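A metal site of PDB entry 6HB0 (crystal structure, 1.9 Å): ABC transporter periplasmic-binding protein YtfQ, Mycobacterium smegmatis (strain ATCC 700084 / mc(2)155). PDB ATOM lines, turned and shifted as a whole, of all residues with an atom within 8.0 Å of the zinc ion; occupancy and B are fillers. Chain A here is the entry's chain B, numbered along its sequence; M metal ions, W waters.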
ATOM      1  N   GLY A 123      20.966  34.722  18.333  1.00  0.00           N
ATOM      2  CA  GLY A 123      20.688  33.945  17.121  1.00  0.00           C
ATOM      3  C   GLY A 123      20.684  32.462  17.446  1.00  0.00           C
ATOM      4  O   GLY A 123      20.899  32.066  18.603  1.00  0.00           O
ATOM      5  N   ALA A 124      20.370  31.658  16.435  1.00  0.00           N
ATOM      6  CA  ALA A 124      20.296  30.227  16.634  1.00  0.00           C
ATOM      7  C   ALA A 124      21.725  29.732  16.780  1.00  0.00           C
ATOM      8  O   ALA A 124      22.625  30.264  16.164  1.00  0.00           O
ATOM      9  CB  ALA A 124      19.609  29.563  15.471  1.00  0.00           C
ATOM     10  N   ASP A 125      21.876  28.715  17.587  1.00  0.00           N
ATOM     11  CA  ASP A 125      23.101  27.929  17.741  1.00  0.00           C
ATOM     12  C   ASP A 125      23.031  26.629  16.892  1.00  0.00           C
ATOM     13  O   ASP A 125      22.436  25.656  17.300  1.00  0.00           O
ATOM     14  CB  ASP A 125      23.211  27.560  19.195  1.00  0.00           C
ATOM     15  CG  ASP A 125      24.550  26.875  19.547  1.00  0.00           C
ATOM     16  OD1 ASP A 125      25.318  26.444  18.629  1.00  0.00           O
ATOM     17  OD2 ASP A 125      24.794  26.813  20.765  1.00  0.00           O
ATOM     18  N   PHE A 126      23.631  26.662  15.718  1.00  0.00           N
ATOM     19  CA  PHE A 126      23.518  25.600  14.761  1.00  0.00           C
ATOM     20  C   PHE A 126      24.332  24.366  15.210  1.00  0.00           C
ATOM     21  O   PHE A 126      23.957  23.271  14.899  1.00  0.00           O
ATOM     22  CB  PHE A 126      24.040  26.070  13.417  1.00  0.00           C
ATOM     23  CG  PHE A 126      23.347  27.295  12.889  1.00  0.00           C
ATOM     24  CD1 PHE A 126      21.980  27.329  12.772  1.00  0.00           C
ATOM     25  CD2 PHE A 126      24.094  28.428  12.499  1.00  0.00           C
ATOM     26  CE1 PHE A 126      21.331  28.454  12.270  1.00  0.00           C
ATOM     27  CE2 PHE A 126      23.451  29.579  12.030  1.00  0.00           C
ATOM     28  CZ  PHE A 126      22.074  29.577  11.916  1.00  0.00           C
ATOM     29  N   ILE A 127      25.426  24.560  15.931  1.00  0.00           N
ATOM     30  CA  ILE A 127      26.185  23.410  16.508  1.00  0.00           C
ATOM     31  C   ILE A 127      25.285  22.671  17.444  1.00  0.00           C
ATOM     32  O   ILE A 127      25.149  21.456  17.372  1.00  0.00           O
ATOM     33  CB  ILE A 127      27.469  23.839  17.232  1.00  0.00           C
ATOM     34  CG1 ILE A 127      28.410  24.488  16.223  1.00  0.00           C
ATOM     35  CG2 ILE A 127      28.079  22.635  17.953  1.00  0.00           C
ATOM     36  CD1 ILE A 127      29.826  24.789  16.718  1.00  0.00           C
ATOM     37  N   GLU A 128      24.610  23.392  18.301  1.00  0.00           N
ATOM     38  CA  GLU A 128      23.714  22.790  19.272  1.00  0.00           C
ATOM     39  C   GLU A 128      22.596  22.035  18.573  1.00  0.00           C
ATOM     40  O   GLU A 128      22.190  20.972  19.016  1.00  0.00           O
ATOM     41  CB  GLU A 128      23.141  23.877  20.178  1.00  0.00           C
ATOM     42  CG  GLU A 128      22.122  23.446  21.182  1.00  0.00           C
ATOM     43  CD  GLU A 128      20.847  24.247  20.991  1.00  0.00           C
ATOM     44  OE1 GLU A 128      20.718  25.305  21.616  1.00  0.00           O
ATOM     45  OE2 GLU A 128      19.975  23.825  20.206  1.00  0.00           O
ATOM     46  N   GLU A 129      22.084  22.555  17.452  1.00  0.00           N
ATOM     47  CA  GLU A 129      21.043  21.804  16.688  1.00  0.00           C
ATOM     48  C   GLU A 129      21.561  20.464  16.245  1.00  0.00           C
ATOM     49  O   GLU A 129      20.900  19.460  16.419  1.00  0.00           O
ATOM     50  CB  GLU A 129      20.572  22.549  15.411  1.00  0.00           C
ATOM     51  CG  GLU A 129      19.699  23.733  15.704  1.00  0.00           C
ATOM     52  CD  GLU A 129      19.240  24.520  14.465  1.00  0.00           C
ATOM     53  OE1 GLU A 129      20.089  24.760  13.592  1.00  0.00           O
ATOM     54  OE2 GLU A 129      18.031  24.945  14.411  1.00  0.00           O
ATOM     55  N   ARG A 131      24.089  18.849  17.430  1.00  0.00           N
ATOM     56  CA  ARG A 131      24.312  18.022  18.595  1.00  0.00           C
ATOM     57  C   ARG A 131      23.077  17.355  19.128  1.00  0.00           C
ATOM     58  O   ARG A 131      23.099  16.178  19.502  1.00  0.00           O
ATOM     59  CB  ARG A 131      24.968  18.841  19.722  1.00  0.00           C
ATOM     60  CG  ARG A 131      25.389  17.989  20.909  1.00  0.00           C
ATOM     61  CD  ARG A 131      26.378  18.740  21.778  1.00  0.00           C
ATOM     62  NE  ARG A 131      25.681  19.839  22.317  1.00  0.00           N
ATOM     63  CZ  ARG A 131      25.994  21.121  22.250  1.00  0.00           C
ATOM     64  NH1 ARG A 131      27.144  21.580  21.812  1.00  0.00           N
ATOM     65  NH2 ARG A 131      25.103  21.921  22.766  1.00  0.00           N
ATOM     66  N   ARG A 132      21.987  18.084  19.210  1.00  0.00           N
ATOM     67  CA  ARG A 132      20.751  17.472  19.680  1.00  0.00           C
ATOM     68  C   ARG A 132      20.206  16.407  18.697  1.00  0.00           C
ATOM     69  O   ARG A 132      19.658  15.386  19.113  1.00  0.00           O
ATOM     70  CB  ARG A 132      19.731  18.561  20.005  1.00  0.00           C
ATOM     71  CG  ARG A 132      20.150  19.480  21.167  1.00  0.00           C
ATOM     72  CD  ARG A 132      19.524  20.897  21.070  1.00  0.00           C
ATOM     73  NE  ARG A 132      18.136  20.700  20.984  1.00  0.00           N
ATOM     74  CZ  ARG A 132      17.236  21.350  20.278  1.00  0.00           C
ATOM     75  NH1 ARG A 132      17.478  22.462  19.602  1.00  0.00           N
ATOM     76  NH2 ARG A 132      16.028  20.850  20.325  1.00  0.00           N
ATOM     77  N   GLU A 262      14.990  22.085  16.523  1.00  0.00           N
ATOM     78  CA  GLU A 262      15.236  23.446  16.033  1.00  0.00           C
ATOM     79  C   GLU A 262      15.754  24.272  17.155  1.00  0.00           C
ATOM     80  O   GLU A 262      15.325  24.102  18.253  1.00  0.00           O
ATOM     81  CB  GLU A 262      13.973  24.085  15.453  1.00  0.00           C
ATOM     82  CG  GLU A 262      14.275  25.431  14.842  1.00  0.00           C
ATOM     83  CD  GLU A 262      13.079  26.137  14.197  1.00  0.00           C
ATOM     84  OE1 GLU A 262      12.149  25.483  13.687  1.00  0.00           O
ATOM     85  OE2 GLU A 262      13.148  27.363  14.147  1.00  0.00           O
ATOM     86  N   CYS A 263      16.729  25.136  16.855  1.00  0.00           N
ATOM     87  CA  CYS A 263      17.149  26.177  17.771  1.00  0.00           C
ATOM     88  C   CYS A 263      16.574  27.437  17.168  1.00  0.00           C
ATOM     89  O   CYS A 263      16.862  27.775  16.018  1.00  0.00           O
ATOM     90  CB  CYS A 263      18.666  26.259  17.848  1.00  0.00           C
ATOM     91  SG  CYS A 263      19.215  27.510  19.030  1.00  0.00           S
ATOM     92  N   ASN A 264      15.727  28.139  17.923  1.00  0.00           N
ATOM     93  CA  ASN A 264      15.054  29.326  17.366  1.00  0.00           C
ATOM     94  C   ASN A 264      16.005  30.494  17.030  1.00  0.00           C
ATOM     95  O   ASN A 264      17.047  30.691  17.654  1.00  0.00           O
ATOM     96  CB  ASN A 264      14.031  29.888  18.361  1.00  0.00           C
ATOM     97  CG  ASN A 264      12.786  29.007  18.535  1.00  0.00           C
ATOM     98  OD1 ASN A 264      12.079  29.186  19.503  1.00  0.00           O
ATOM     99  ND2 ASN A 264      12.515  28.091  17.608  1.00  0.00           N
ATOM    100  N   PRO A 265      15.654  31.281  16.027  1.00  0.00           N
ATOM    101  CA  PRO A 265      16.306  32.560  15.881  1.00  0.00           C
ATOM    102  C   PRO A 265      15.865  33.553  16.983  1.00  0.00           C
ATOM    103  O   PRO A 265      15.107  33.198  17.888  1.00  0.00           O
ATOM    104  CB  PRO A 265      15.800  33.013  14.508  1.00  0.00           C
ATOM    105  CG  PRO A 265      14.413  32.526  14.484  1.00  0.00           C
ATOM    106  CD  PRO A 265      14.464  31.184  15.173  1.00  0.00           C
ATOM    107  N   ARG A 287      25.994  35.493  24.549  1.00  0.00           N
ATOM    108  CA  ARG A 287      25.089  34.861  23.617  1.00  0.00           C
ATOM    109  C   ARG A 287      23.802  34.558  24.336  1.00  0.00           C
ATOM    110  O   ARG A 287      23.806  33.915  25.356  1.00  0.00           O
ATOM    111  CB  ARG A 287      25.679  33.557  23.172  1.00  0.00           C
ATOM    112  CG  ARG A 287      26.364  33.604  21.835  1.00  0.00           C
ATOM    113  CD  ARG A 287      25.443  32.877  20.873  1.00  0.00           C
ATOM    114  NE  ARG A 287      26.161  32.168  19.853  1.00  0.00           N
ATOM    115  CZ  ARG A 287      25.560  31.497  18.896  1.00  0.00           C
ATOM    116  NH1 ARG A 287      26.317  30.882  18.034  1.00  0.00           N
ATOM    117  NH2 ARG A 287      24.211  31.441  18.791  1.00  0.00           N
ATOM    118  N   VAL A 288      22.711  35.080  23.855  1.00  0.00           N
ATOM    119  CA  VAL A 288      21.445  34.728  24.422  1.00  0.00           C
ATOM    120  C   VAL A 288      21.206  33.294  24.003  1.00  0.00           C
ATOM    121  O   VAL A 288      21.519  32.907  22.871  1.00  0.00           O
ATOM    122  CB  VAL A 288      20.372  35.639  23.853  1.00  0.00           C
ATOM    123  CG1 VAL A 288      19.005  35.130  24.178  1.00  0.00           C
ATOM    124  CG2 VAL A 288      20.497  36.994  24.470  1.00  0.00           C
ATOM    125  N   VAL A 289      20.627  32.487  24.883  1.00  0.00           N
ATOM    126  CA  VAL A 289      20.189  31.180  24.446  1.00  0.00           C
ATOM    127  C   VAL A 289      18.712  31.272  24.041  1.00  0.00           C
ATOM    128  O   VAL A 289      17.866  31.554  24.874  1.00  0.00           O
ATOM    129  CB  VAL A 289      20.441  30.088  25.505  1.00  0.00           C
ATOM    130  CG1 VAL A 289      21.927  30.115  25.952  1.00  0.00           C
ATOM    131  CG2 VAL A 289      19.485  30.245  26.648  1.00  0.00           C
ATOM    132  N   THR A 290      18.425  31.081  22.756  1.00  0.00           N
ATOM    133  CA  THR A 290      17.057  31.162  22.249  1.00  0.00           C
ATOM    134  C   THR A 290      16.335  29.881  22.640  1.00  0.00           C
ATOM    135  O   THR A 290      16.976  28.937  23.098  1.00  0.00           O
ATOM    136  CB  THR A 290      17.046  31.322  20.713  1.00  0.00           C
ATOM    137  OG1 THR A 290      17.858  30.303  20.104  1.00  0.00           O
ATOM    138  CG2 THR A 290      17.607  32.689  20.342  1.00  0.00           C
ATOM    139  N   PRO A 291      15.021  29.845  22.528  1.00  0.00           N
ATOM    140  CA  PRO A 291      14.322  28.600  22.842  1.00  0.00           C
ATOM    141  C   PRO A 291      14.596  27.494  21.832  1.00  0.00           C
ATOM    142  O   PRO A 291      14.903  27.751  20.626  1.00  0.00           O
ATOM    143  CB  PRO A 291      12.838  28.999  22.794  1.00  0.00           C
ATOM    144  CG  PRO A 291      12.859  30.459  22.998  1.00  0.00           C
ATOM    145  CD  PRO A 291      14.080  30.940  22.277  1.00  0.00           C
ATOM    146  N   ASP A 292      14.505  26.285  22.344  1.00  0.00           N
ATOM    147  CA  ASP A 292      14.705  25.084  21.569  1.00  0.00           C
ATOM    148  C   ASP A 292      13.411  24.322  21.412  1.00  0.00           C
ATOM    149  O   ASP A 292      12.566  24.308  22.289  1.00  0.00           O
ATOM    150  CB  ASP A 292      15.764  24.227  22.267  1.00  0.00           C
ATOM    151  CG  ASP A 292      17.121  24.813  22.191  1.00  0.00           C
ATOM    152  OD1 ASP A 292      17.442  25.537  21.209  1.00  0.00           O
ATOM    153  OD2 ASP A 292      17.912  24.585  23.114  1.00  0.00           O
ATOM    154  N   GLU A 293      13.250  23.729  20.253  1.00  0.00           N
ATOM    155  CA  GLU A 293      12.104  22.908  19.918  1.00  0.00           C
ATOM    156  C   GLU A 293      12.601  21.501  19.584  1.00  0.00           C
ATOM    157  O   GLU A 293      13.718  21.356  19.056  1.00  0.00           O
ATOM    158  CB  GLU A 293      11.410  23.513  18.710  1.00  0.00           C
ATOM    159  CG  GLU A 293      10.806  24.876  18.994  1.00  0.00           C
ATOM    160  CD  GLU A 293       9.975  25.465  17.844  1.00  0.00           C
ATOM    161  OE1 GLU A 293       9.202  24.732  17.184  1.00  0.00           O
ATOM    162  OE2 GLU A 293      10.062  26.681  17.627  1.00  0.00           O
HETATM  163 ZN    ZN M   1      19.167  26.426  20.911  1.00  0.00          ZN
HETATM  164  O   HOH W   1      19.376  27.735  22.450  1.00  0.00           O
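The guanidinium group (NH1) of Arg 132 lies within salt-bridge range of the side-chain carboxylate (OE2) of Glu 128 (2.9 Å).
OE2 of Glu 129 sits at hydrogen-bond distance from N of Cys 263 (2.8 Å).
The side-chain carboxylate (OD1) of Asp 292 lies close to the guanidinium group (NH1) of Arg 132.
The side-chain sulfur (SG) of Cys 263 sits close to the side-chain hydroxyl (OG1) of Thr 290, 3.3 Å away.
The side-chain carboxylate (OD1) of Asp 125 sits at hydrogen-bond distance from the backbone NH (N) of Glu 128 (3.2 Å).
SG of Cys 263 lies close to N of Asp 125 (3.3 Å).
The side-chain hydroxyl (OG1) of Thr 290 is in hydrogen-bond range of the backbone carbonyl oxygen (O) of Asn 264 (2.6 Å).
O of Thr 290 touches the zinc ion, 3.99 Å away.
Four residues have an atom within 4 Å of the zinc ion: Glu 128, Cys 263, Thr 290 and Asp 292.
The zinc ion is bound by the side-chain carboxylate (OD1) of Asp 292 (2.0 Å), water W1 (2.0 Å), the side-chain carboxylate (OE1) of Glu 128 (2.0 Å) and the side-chain sulfur (SG) of Cys 263 (2.2 Å).
Slightly farther from the zinc ion lies OE2 of Glu 128 (2.8 Å).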
